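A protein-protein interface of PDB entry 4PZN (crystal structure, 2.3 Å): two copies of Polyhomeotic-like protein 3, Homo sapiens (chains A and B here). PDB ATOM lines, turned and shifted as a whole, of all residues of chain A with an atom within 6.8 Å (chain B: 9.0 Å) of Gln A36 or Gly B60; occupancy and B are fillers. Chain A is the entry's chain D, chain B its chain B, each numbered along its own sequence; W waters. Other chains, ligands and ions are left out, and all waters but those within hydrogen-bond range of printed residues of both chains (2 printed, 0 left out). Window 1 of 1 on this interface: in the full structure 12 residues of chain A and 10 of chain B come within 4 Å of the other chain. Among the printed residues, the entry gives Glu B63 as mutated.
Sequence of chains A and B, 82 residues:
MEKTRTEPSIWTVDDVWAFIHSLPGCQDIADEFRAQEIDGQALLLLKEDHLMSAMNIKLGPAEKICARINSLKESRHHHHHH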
ATOM      1  N   VAL A  13      16.752   5.170  -9.056  1.00  0.00           N
ATOM      2  CA  VAL A  13      17.015   5.003 -10.474  1.00  0.00           C
ATOM      3  C   VAL A  13      18.418   4.400 -10.650  1.00  0.00           C
ATOM      4  O   VAL A  13      18.644   3.561 -11.521  1.00  0.00           O
ATOM      5  CB  VAL A  13      16.898   6.338 -11.221  1.00  0.00           C
ATOM      6  CG1 VAL A  13      17.559   6.249 -12.587  1.00  0.00           C
ATOM      7  CG2 VAL A  13      15.441   6.708 -11.390  1.00  0.00           C
ATOM      8  N   ASP A  31      20.787   1.452 -19.747  1.00  0.00           N
ATOM      9  CA  ASP A  31      20.816   2.888 -19.993  1.00  0.00           C
ATOM     10  C   ASP A  31      19.427   3.378 -20.351  1.00  0.00           C
ATOM     11  O   ASP A  31      19.053   4.497 -20.042  1.00  0.00           O
ATOM     12  CB  ASP A  31      21.776   3.216 -21.131  1.00  0.00           C
ATOM     13  CG  ASP A  31      23.196   2.923 -20.780  1.00  0.00           C
ATOM     14  OD1 ASP A  31      23.558   3.115 -19.604  1.00  0.00           O
ATOM     15  OD2 ASP A  31      23.935   2.464 -21.674  1.00  0.00           O
ATOM     16  N   GLU A  32      18.660   2.507 -20.981  1.00  0.00           N
ATOM     17  CA  GLU A  32      17.309   2.856 -21.339  1.00  0.00           C
ATOM     18  C   GLU A  32      16.457   2.915 -20.083  1.00  0.00           C
ATOM     19  O   GLU A  32      15.606   3.788 -19.948  1.00  0.00           O
ATOM     20  CB  GLU A  32      16.743   1.846 -22.338  1.00  0.00           C
ATOM     21  CG  GLU A  32      15.412   2.249 -22.907  1.00  0.00           C
ATOM     22  CD  GLU A  32      15.484   3.533 -23.709  1.00  0.00           C
ATOM     23  OE1 GLU A  32      16.593   3.853 -24.209  1.00  0.00           O
ATOM     24  OE2 GLU A  32      14.436   4.220 -23.818  1.00  0.00           O
ATOM     25  N   PHE A  33      16.731   2.026 -19.133  1.00  0.00           N
ATOM     26  CA  PHE A  33      16.007   2.054 -17.871  1.00  0.00           C
ATOM     27  C   PHE A  33      16.265   3.352 -17.123  1.00  0.00           C
ATOM     28  O   PHE A  33      15.330   3.965 -16.614  1.00  0.00           O
ATOM     29  CB  PHE A  33      16.380   0.856 -16.996  1.00  0.00           C
ATOM     30  CG  PHE A  33      15.572  -0.375 -17.283  1.00  0.00           C
ATOM     31  CD1 PHE A  33      15.658  -1.010 -18.510  1.00  0.00           C
ATOM     32  CD2 PHE A  33      14.706  -0.885 -16.334  1.00  0.00           C
ATOM     33  CE1 PHE A  33      14.918  -2.144 -18.771  1.00  0.00           C
ATOM     34  CE2 PHE A  33      13.960  -2.015 -16.592  1.00  0.00           C
ATOM     35  CZ  PHE A  33      14.066  -2.648 -17.815  1.00  0.00           C
ATOM     36  N   ARG A  34      17.503   3.829 -17.141  1.00  0.00           N
ATOM     37  CA  ARG A  34      17.828   5.045 -16.404  1.00  0.00           C
ATOM     38  C   ARG A  34      17.276   6.274 -17.112  1.00  0.00           C
ATOM     39  O   ARG A  34      16.830   7.228 -16.478  1.00  0.00           O
ATOM     40  CB  ARG A  34      19.339   5.169 -16.199  1.00  0.00           C
ATOM     41  CG  ARG A  34      19.778   6.491 -15.565  1.00  0.00           C
ATOM     42  CD  ARG A  34      21.295   6.554 -15.369  1.00  0.00           C
ATOM     43  NE  ARG A  34      21.657   6.084 -14.031  1.00  0.00           N
ATOM     44  CZ  ARG A  34      22.856   5.612 -13.673  1.00  0.00           C
ATOM     45  NH1 ARG A  34      23.850   5.525 -14.557  1.00  0.00           N
ATOM     46  NH2 ARG A  34      23.056   5.220 -12.420  1.00  0.00           N
ATOM     47  N   ALA A  35      17.280   6.228 -18.432  1.00  0.00           N
ATOM     48  CA  ALA A  35      16.773   7.319 -19.218  1.00  0.00           C
ATOM     49  C   ALA A  35      15.273   7.467 -19.008  1.00  0.00           C
ATOM     50  O   ALA A  35      14.746   8.570 -19.090  1.00  0.00           O
ATOM     51  CB  ALA A  35      17.087   7.086 -20.676  1.00  0.00           C
ATOM     52  N   GLN A  36      14.611   6.364 -18.655  1.00  0.00           N
ATOM     53  CA  GLN A  36      13.160   6.344 -18.447  1.00  0.00           C
ATOM     54  C   GLN A  36      12.845   6.602 -16.983  1.00  0.00           C
ATOM     55  O   GLN A  36      11.689   6.539 -16.573  1.00  0.00           O
ATOM     56  CB  GLN A  36      12.550   5.000 -18.864  1.00  0.00           C
ATOM     57  CG  GLN A  36      12.527   4.697 -20.352  1.00  0.00           C
ATOM     58  CD  GLN A  36      11.560   5.567 -21.158  1.00  0.00           C
ATOM     59  OE1 GLN A  36      10.758   6.333 -20.613  1.00  0.00           O
ATOM     60  NE2 GLN A  36      11.631   5.433 -22.476  1.00  0.00           N
ATOM     61  N   GLU A  37      13.895   6.845 -16.207  1.00  0.00           N
ATOM     62  CA  GLU A  37      13.791   7.173 -14.789  1.00  0.00           C
ATOM     63  C   GLU A  37      12.990   6.102 -14.060  1.00  0.00           C
ATOM     64  O   GLU A  37      12.121   6.413 -13.234  1.00  0.00           O
ATOM     65  CB  GLU A  37      13.158   8.546 -14.588  1.00  0.00           C
ATOM     66  CG  GLU A  37      14.040   9.701 -15.008  1.00  0.00           C
ATOM     67  CD  GLU A  37      13.327  11.034 -14.907  1.00  0.00           C
ATOM     68  OE1 GLU A  37      12.323  11.125 -14.165  1.00  0.00           O
ATOM     69  OE2 GLU A  37      13.758  11.993 -15.574  1.00  0.00           O
ATOM     70  N   ILE A  38      13.299   4.846 -14.380  1.00  0.00           N
ATOM     71  CA  ILE A  38      12.685   3.697 -13.741  1.00  0.00           C
ATOM     72  C   ILE A  38      13.394   3.403 -12.418  1.00  0.00           C
ATOM     73  O   ILE A  38      14.549   2.990 -12.406  1.00  0.00           O
ATOM     74  CB  ILE A  38      12.758   2.464 -14.666  1.00  0.00           C
ATOM     75  CG1 ILE A  38      11.845   2.682 -15.881  1.00  0.00           C
ATOM     76  CG2 ILE A  38      12.377   1.192 -13.931  1.00  0.00           C
ATOM     77  CD1 ILE A  38      11.883   1.582 -16.883  1.00  0.00           C
ATOM     78  N   ASP A  39      12.686   3.586 -11.309  1.00  0.00           N
ATOM     79  CA  ASP A  39      13.224   3.263  -9.997  1.00  0.00           C
ATOM     80  C   ASP A  39      12.581   1.976  -9.575  1.00  0.00           C
ATOM     81  O   ASP A  39      11.884   1.346 -10.372  1.00  0.00           O
ATOM     82  CB  ASP A  39      12.969   4.363  -8.953  1.00  0.00           C
ATOM     83  CG  ASP A  39      11.500   4.821  -8.903  1.00  0.00           C
ATOM     84  OD1 ASP A  39      10.609   4.211  -9.542  1.00  0.00           O
ATOM     85  OD2 ASP A  39      11.236   5.784  -8.175  1.00  0.00           O
ATOM     86  N   GLN A  41      10.103   1.279  -7.561  1.00  0.00           N
ATOM     87  CA  GLN A  41       8.655   1.240  -7.568  1.00  0.00           C
ATOM     88  C   GLN A  41       8.152   0.985  -8.975  1.00  0.00           C
ATOM     89  O   GLN A  41       7.381   0.065  -9.188  1.00  0.00           O
ATOM     90  CB  GLN A  41       8.084   2.547  -7.055  1.00  0.00           C
ATOM     91  CG  GLN A  41       6.594   2.498  -6.895  1.00  0.00           C
ATOM     92  CD  GLN A  41       6.032   3.826  -6.468  1.00  0.00           C
ATOM     93  OE1 GLN A  41       6.774   4.701  -5.998  1.00  0.00           O
ATOM     94  NE2 GLN A  41       4.708   3.980  -6.591  1.00  0.00           N
ATOM     95  N   ALA A  42       8.698   1.702  -9.950  1.00  0.00           N
ATOM     96  CA  ALA A  42       8.313   1.491 -11.341  1.00  0.00           C
ATOM     97  C   ALA A  42       8.746   0.112 -11.819  1.00  0.00           C
ATOM     98  O   ALA A  42       7.999  -0.570 -12.522  1.00  0.00           O
ATOM     99  CB  ALA A  42       8.902   2.571 -12.233  1.00  0.00           C
ATOM    100  N   LEU A  43       9.955  -0.298 -11.447  1.00  0.00           N
ATOM    101  CA  LEU A  43      10.469  -1.596 -11.885  1.00  0.00           C
ATOM    102  C   LEU A  43       9.513  -2.764 -11.574  1.00  0.00           C
ATOM    103  O   LEU A  43       9.299  -3.647 -12.394  1.00  0.00           O
ATOM    104  CB  LEU A  43      11.833  -1.850 -11.236  1.00  0.00           C
ATOM    105  CG  LEU A  43      12.528  -3.122 -11.685  1.00  0.00           C
ATOM    106  CD1 LEU A  43      13.122  -2.907 -13.052  1.00  0.00           C
ATOM    107  CD2 LEU A  43      13.616  -3.515 -10.665  1.00  0.00           C
ATOM    108  N   LEU A  46       6.344  -2.903 -13.838  1.00  0.00           N
ATOM    109  CA  LEU A  46       6.553  -3.204 -15.251  1.00  0.00           C
ATOM    110  C   LEU A  46       5.959  -4.536 -15.669  1.00  0.00           C
ATOM    111  O   LEU A  46       5.836  -5.458 -14.873  1.00  0.00           O
ATOM    112  CB  LEU A  46       8.047  -3.221 -15.601  1.00  0.00           C
ATOM    113  CG  LEU A  46       8.743  -1.869 -15.602  1.00  0.00           C
ATOM    114  CD1 LEU A  46      10.218  -2.033 -15.880  1.00  0.00           C
ATOM    115  CD2 LEU A  46       8.064  -0.957 -16.614  1.00  0.00           C
ATOM    116  N   ALA A  54       7.958   0.856 -24.745  1.00  0.00           N
ATOM    117  CA  ALA A  54       8.752   2.057 -24.496  1.00  0.00           C
ATOM    118  C   ALA A  54      10.242   1.845 -24.700  1.00  0.00           C
ATOM    119  O   ALA A  54      11.006   2.817 -24.804  1.00  0.00           O
ATOM    120  CB  ALA A  54       8.493   2.573 -23.103  1.00  0.00           C
ATOM    121  N   MET A  55      10.674   0.587 -24.667  1.00  0.00           N
ATOM    122  CA  MET A  55      12.097   0.302 -24.803  1.00  0.00           C
ATOM    123  C   MET A  55      12.506  -0.630 -25.940  1.00  0.00           C
ATOM    124  O   MET A  55      13.660  -1.037 -25.998  1.00  0.00           O
ATOM    125  CB  MET A  55      12.611  -0.261 -23.490  1.00  0.00           C
ATOM    126  CG  MET A  55      12.432   0.716 -22.370  1.00  0.00           C
ATOM    127  SD  MET A  55      13.335   0.209 -20.922  1.00  0.00           S
ATOM    128  CE  MET A  55      11.986  -0.526 -20.004  1.00  0.00           C
ATOM    129  N   PRO B  24       5.431  13.644  -6.042  1.00  0.00           N
ATOM    130  CA  PRO B  24       6.884  13.791  -6.200  1.00  0.00           C
ATOM    131  C   PRO B  24       7.283  13.906  -7.674  1.00  0.00           C
ATOM    132  O   PRO B  24       6.820  13.084  -8.482  1.00  0.00           O
ATOM    133  CB  PRO B  24       7.436  12.495  -5.590  1.00  0.00           C
ATOM    134  CG  PRO B  24       6.428  12.097  -4.559  1.00  0.00           C
ATOM    135  CD  PRO B  24       5.083  12.523  -5.151  1.00  0.00           C
ATOM    136  N   CYS B  26       6.288  15.816  -9.976  1.00  0.00           N
ATOM    137  CA  CYS B  26       5.217  16.098 -10.934  1.00  0.00           C
ATOM    138  C   CYS B  26       4.805  17.559 -11.075  1.00  0.00           C
ATOM    139  O   CYS B  26       3.759  17.845 -11.642  1.00  0.00           O
ATOM    140  CB  CYS B  26       3.996  15.253 -10.604  1.00  0.00           C
ATOM    141  SG  CYS B  26       4.322  13.508 -10.908  1.00  0.00           S
ATOM    142  N   ILE B  29       4.783  18.364 -14.738  1.00  0.00           N
ATOM    143  CA  ILE B  29       3.901  17.401 -15.378  1.00  0.00           C
ATOM    144  C   ILE B  29       2.429  17.738 -15.085  1.00  0.00           C
ATOM    145  O   ILE B  29       1.539  17.441 -15.891  1.00  0.00           O
ATOM    146  CB  ILE B  29       4.242  15.967 -14.876  1.00  0.00           C
ATOM    147  CG1 ILE B  29       5.511  15.426 -15.541  1.00  0.00           C
ATOM    148  CG2 ILE B  29       3.100  14.998 -15.059  1.00  0.00           C
ATOM    149  CD1 ILE B  29       6.075  14.178 -14.862  1.00  0.00           C
ATOM    150  N   GLU B  48      -0.954   4.160 -19.094  1.00  0.00           N
ATOM    151  CA  GLU B  48       0.457   4.502 -19.218  1.00  0.00           C
ATOM    152  C   GLU B  48       0.812   4.993 -20.613  1.00  0.00           C
ATOM    153  O   GLU B  48       1.572   5.951 -20.789  1.00  0.00           O
ATOM    154  CB  GLU B  48       1.323   3.294 -18.856  1.00  0.00           C
ATOM    155  CG  GLU B  48       1.153   2.812 -17.434  1.00  0.00           C
ATOM    156  CD  GLU B  48       0.008   1.844 -17.285  1.00  0.00           C
ATOM    157  OE1 GLU B  48      -0.490   1.361 -18.316  1.00  0.00           O
ATOM    158  OE2 GLU B  48      -0.389   1.554 -16.139  1.00  0.00           O
ATOM    159  N   LEU B  51      -0.014   8.599 -21.254  1.00  0.00           N
ATOM    160  CA  LEU B  51       0.917   9.512 -20.599  1.00  0.00           C
ATOM    161  C   LEU B  51       2.210   9.632 -21.379  1.00  0.00           C
ATOM    162  O   LEU B  51       2.792  10.723 -21.472  1.00  0.00           O
ATOM    163  CB  LEU B  51       1.233   9.079 -19.157  1.00  0.00           C
ATOM    164  CG  LEU B  51       0.260   9.432 -18.024  1.00  0.00           C
ATOM    165  CD1 LEU B  51      -1.063   8.712 -18.119  1.00  0.00           C
ATOM    166  CD2 LEU B  51       0.923   9.229 -16.639  1.00  0.00           C
ATOM    167  N   MET B  52       2.689   8.508 -21.903  1.00  0.00           N
ATOM    168  CA  MET B  52       3.935   8.530 -22.652  1.00  0.00           C
ATOM    169  C   MET B  52       3.719   9.141 -24.036  1.00  0.00           C
ATOM    170  O   MET B  52       4.477  10.017 -24.449  1.00  0.00           O
ATOM    171  CB  MET B  52       4.512   7.122 -22.782  1.00  0.00           C
ATOM    172  CG  MET B  52       4.804   6.433 -21.455  1.00  0.00           C
ATOM    173  SD  MET B  52       5.831   4.958 -21.695  1.00  0.00           S
ATOM    174  CE  MET B  52       4.607   3.669 -21.932  1.00  0.00           C
ATOM    175  N   ASN B  56       4.158  12.845 -23.353  1.00  0.00           N
ATOM    176  CA  ASN B  56       5.606  12.726 -23.384  1.00  0.00           C
ATOM    177  C   ASN B  56       6.231  12.375 -22.024  1.00  0.00           C
ATOM    178  O   ASN B  56       7.382  12.703 -21.762  1.00  0.00           O
ATOM    179  CB  ASN B  56       6.232  14.008 -23.932  1.00  0.00           C
ATOM    180  CG  ASN B  56       7.637  13.779 -24.466  1.00  0.00           C
ATOM    181  OD1 ASN B  56       7.925  12.718 -25.022  1.00  0.00           O
ATOM    182  ND2 ASN B  56       8.522  14.755 -24.274  1.00  0.00           N
ATOM    183  N   ILE B  57       5.449  11.792 -21.124  1.00  0.00           N
ATOM    184  CA  ILE B  57       5.955  11.434 -19.797  1.00  0.00           C
ATOM    185  C   ILE B  57       6.753  10.134 -19.882  1.00  0.00           C
ATOM    186  O   ILE B  57       6.344   9.203 -20.577  1.00  0.00           O
ATOM    187  CB  ILE B  57       4.798  11.274 -18.800  1.00  0.00           C
ATOM    188  CG1 ILE B  57       3.974  12.574 -18.746  1.00  0.00           C
ATOM    189  CG2 ILE B  57       5.320  10.855 -17.431  1.00  0.00           C
ATOM    190  CD1 ILE B  57       2.666  12.464 -17.980  1.00  0.00           C
ATOM    191  N   LYS B  58       7.849  10.032 -19.137  1.00  0.00           N
ATOM    192  CA  LYS B  58       8.668   8.823 -19.179  1.00  0.00           C
ATOM    193  C   LYS B  58       8.026   7.673 -18.416  1.00  0.00           C
ATOM    194  O   LYS B  58       7.143   7.875 -17.577  1.00  0.00           O
ATOM    195  CB  LYS B  58      10.056   9.099 -18.603  1.00  0.00           C
ATOM    196  CG  LYS B  58      10.915   9.982 -19.487  1.00  0.00           C
ATOM    197  CD  LYS B  58      12.076  10.470 -18.688  1.00  0.00           C
ATOM    198  CE  LYS B  58      12.994  11.358 -19.473  1.00  0.00           C
ATOM    199  NZ  LYS B  58      14.031  11.814 -18.499  1.00  0.00           N
ATOM    200  N   LEU B  59       8.478   6.462 -18.727  1.00  0.00           N
ATOM    201  CA  LEU B  59       7.781   5.256 -18.296  1.00  0.00           C
ATOM    202  C   LEU B  59       7.817   5.116 -16.766  1.00  0.00           C
ATOM    203  O   LEU B  59       6.845   4.678 -16.170  1.00  0.00           O
ATOM    204  CB  LEU B  59       8.380   4.025 -18.972  1.00  0.00           C
ATOM    205  CG  LEU B  59       7.828   2.661 -18.546  1.00  0.00           C
ATOM    206  CD1 LEU B  59       6.350   2.567 -18.915  1.00  0.00           C
ATOM    207  CD2 LEU B  59       8.614   1.513 -19.184  1.00  0.00           C
ATOM    208  N   GLY B  60       8.926   5.480 -16.130  1.00  0.00           N
ATOM    209  CA  GLY B  60       8.994   5.391 -14.678  1.00  0.00           C
ATOM    210  C   GLY B  60       7.940   6.262 -14.000  1.00  0.00           C
ATOM    211  O   GLY B  60       7.059   5.760 -13.285  1.00  0.00           O
ATOM    212  N   PRO B  61       7.981   7.573 -14.268  1.00  0.00           N
ATOM    213  CA  PRO B  61       6.927   8.450 -13.741  1.00  0.00           C
ATOM    214  C   PRO B  61       5.519   8.032 -14.187  1.00  0.00           C
ATOM    215  O   PRO B  61       4.601   8.109 -13.372  1.00  0.00           O
ATOM    216  CB  PRO B  61       7.289   9.805 -14.342  1.00  0.00           C
ATOM    217  CG  PRO B  61       8.790   9.735 -14.492  1.00  0.00           C
ATOM    218  CD  PRO B  61       9.023   8.338 -14.977  1.00  0.00           C
ATOM    219  N   ALA B  62       5.358   7.579 -15.434  1.00  0.00           N
ATOM    220  CA  ALA B  62       4.037   7.158 -15.918  1.00  0.00           C
ATOM    221  C   ALA B  62       3.498   5.982 -15.116  1.00  0.00           C
ATOM    222  O   ALA B  62       2.305   5.895 -14.860  1.00  0.00           O
ATOM    223  CB  ALA B  62       4.077   6.799 -17.427  1.00  0.00           C
ATOM    224  N   GLU B  63       4.373   5.070 -14.724  1.00  0.00           N
ATOM    225  CA  GLU B  63       3.938   3.895 -13.977  1.00  0.00           C
ATOM    226  C   GLU B  63       3.490   4.328 -12.581  1.00  0.00           C
ATOM    227  O   GLU B  63       2.458   3.898 -12.066  1.00  0.00           O
ATOM    228  CB  GLU B  63       5.090   2.896 -13.827  1.00  0.00           C
ATOM    229  CG  GLU B  63       5.501   2.209 -15.100  1.00  0.00           C
ATOM    230  CD  GLU B  63       4.654   1.022 -15.443  1.00  0.00           C
ATOM    231  OE1 GLU B  63       3.631   0.774 -14.773  1.00  0.00           O
ATOM    232  OE2 GLU B  63       4.997   0.354 -16.430  1.00  0.00           O
ATOM    233  N   LYS B  64       4.274   5.218 -11.993  1.00  0.00           N
ATOM    234  CA  LYS B  64       4.030   5.637 -10.633  1.00  0.00           C
ATOM    235  C   LYS B  64       2.788   6.525 -10.557  1.00  0.00           C
ATOM    236  O   LYS B  64       2.016   6.425  -9.610  1.00  0.00           O
ATOM    237  CB  LYS B  64       5.271   6.319 -10.067  1.00  0.00           C
ATOM    238  CG  LYS B  64       6.431   5.335  -9.828  1.00  0.00           C
ATOM    239  CD  LYS B  64       7.624   5.970  -9.060  1.00  0.00           C
ATOM    240  CE  LYS B  64       8.612   6.673  -9.982  1.00  0.00           C
ATOM    241  NZ  LYS B  64       9.556   7.553  -9.209  1.00  0.00           N
ATOM    242  N   ILE B  65       2.611   7.402 -11.543  1.00  0.00           N
ATOM    243  CA  ILE B  65       1.393   8.211 -11.628  1.00  0.00           C
ATOM    244  C   ILE B  65       0.159   7.340 -11.792  1.00  0.00           C
ATOM    245  O   ILE B  65      -0.814   7.500 -11.068  1.00  0.00           O
ATOM    246  CB  ILE B  65       1.472   9.223 -12.773  1.00  0.00           C
ATOM    247  CG1 ILE B  65       2.494  10.306 -12.408  1.00  0.00           C
ATOM    248  CG2 ILE B  65       0.108   9.873 -12.999  1.00  0.00           C
ATOM    249  CD1 ILE B  65       2.855  11.238 -13.535  1.00  0.00           C
ATOM    250  N   CYS B  66       0.220   6.370 -12.698  1.00  0.00           N
ATOM    251  CA  CYS B  66      -0.924   5.509 -12.889  1.00  0.00           C
ATOM    252  C   CYS B  66      -1.216   4.710 -11.626  1.00  0.00           C
ATOM    253  O   CYS B  66      -2.375   4.431 -11.323  1.00  0.00           O
ATOM    254  CB  CYS B  66      -0.694   4.579 -14.082  1.00  0.00           C
ATOM    255  SG  CYS B  66      -0.797   5.448 -15.682  1.00  0.00           S
ATOM    256  N   ALA B  67      -0.171   4.392 -10.860  1.00  0.00           N
ATOM    257  CA  ALA B  67      -0.357   3.669  -9.613  1.00  0.00           C
ATOM    258  C   ALA B  67      -1.063   4.562  -8.591  1.00  0.00           C
ATOM    259  O   ALA B  67      -1.948   4.106  -7.885  1.00  0.00           O
ATOM    260  CB  ALA B  67       0.977   3.169  -9.074  1.00  0.00           C
HETATM  261  O   HOH W   1      11.362   7.952 -11.357  1.00  0.00           O
HETATM  262  O   HOH W   2       2.818   5.741  -6.955  1.00  0.00           O
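No position is printed for both chains.
Of the 15 pairs that touch across the chains among the printed residues, none has its exchanged pair printed and touching as well.
Water W1 lies within hydrogen-bond range of the backbone carbonyl oxygen of Glu A37 (2.5 Å) and the side-chain amino group of Lys B64 (2.8 Å).
Water W2 lies within hydrogen-bond range of the side-chain amide nitrogen of Gln A41 (2.6 Å) and the backbone carbonyl oxygen of Lys B64 (2.9 Å).
OE1 of Gln A36 touches CB of Lys B58 (3.5 Å).
Gln A36 touches Pro B61.
O of Glu A37 touches CA of Gly B60 (3.6 Å).
Glu A37 touches Pro B61 (OE1 to CG, 3.8 Å).
Leu B59 touches Ile A38 (CD2 to CD1, 3.998 Å).
Gln A41 touches Lys B64 (OE1 to CD, 3.4 Å).
CB of Ala A42 touches CA of Gly B60, 3.7 Å away.
Leu B59 touches Leu A46.
Glu B63 touches Leu A46 (OE2 to CD2, 3.3 Å).
Ala A54 touches Met B52.
OE2 of Glu A32 sits at hydrogen-bond distance from NE2 of Gln A36 (3.3 Å).
OD1 of Asp A39 is in hydrogen-bond range of N of Ala A42, at 3.2 Å.
The backbone NH of Ile A38 sits at hydrogen-bond distance from the backbone carbonyl oxygen of Phe A33 (3.1 Å).
Hydrophobic or aromatic side chains of chain B that line the printed part of chain A: Met B52, Leu B59 and Pro B61.
The side-chain amino group (NZ) of Lys B58 is in salt-bridge range of the side-chain carboxylate (OE2) of Glu A37, at 2.9 Å.
OE1 of Gln A36 is in hydrogen-bond range of N of Leu B59 (3.0 Å).
The side-chain carboxylate (OD2) of Asp A39 lies within salt-bridge range of the side-chain amino group (NZ) of Lys B64 (2.6 Å).
The side-chain amino group (NZ) of Lys B58 sits close to the backbone carbonyl oxygen (O) of Ala A35 (3.4 Å).
N of Gly B60 is in hydrogen-bond range of O of Gln A36, 3.0 Å away.
Gly B60 touches three residues of chain A.
Ala A35 touches one residue of chain B.
Of the printed residues of chain B, Ala A42 touches Gly B60.
Of the printed residues of chain A, Met B52 touches Ala A54.
Printed residues of chain A within 4 Å of Glu B63: Leu A46.
Printed residues of chain B within 4 Å of Asp A39: Lys B64.
The nearest residue of chain A that does not touch Gly B60 is Ile A38 (4.1 Å).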
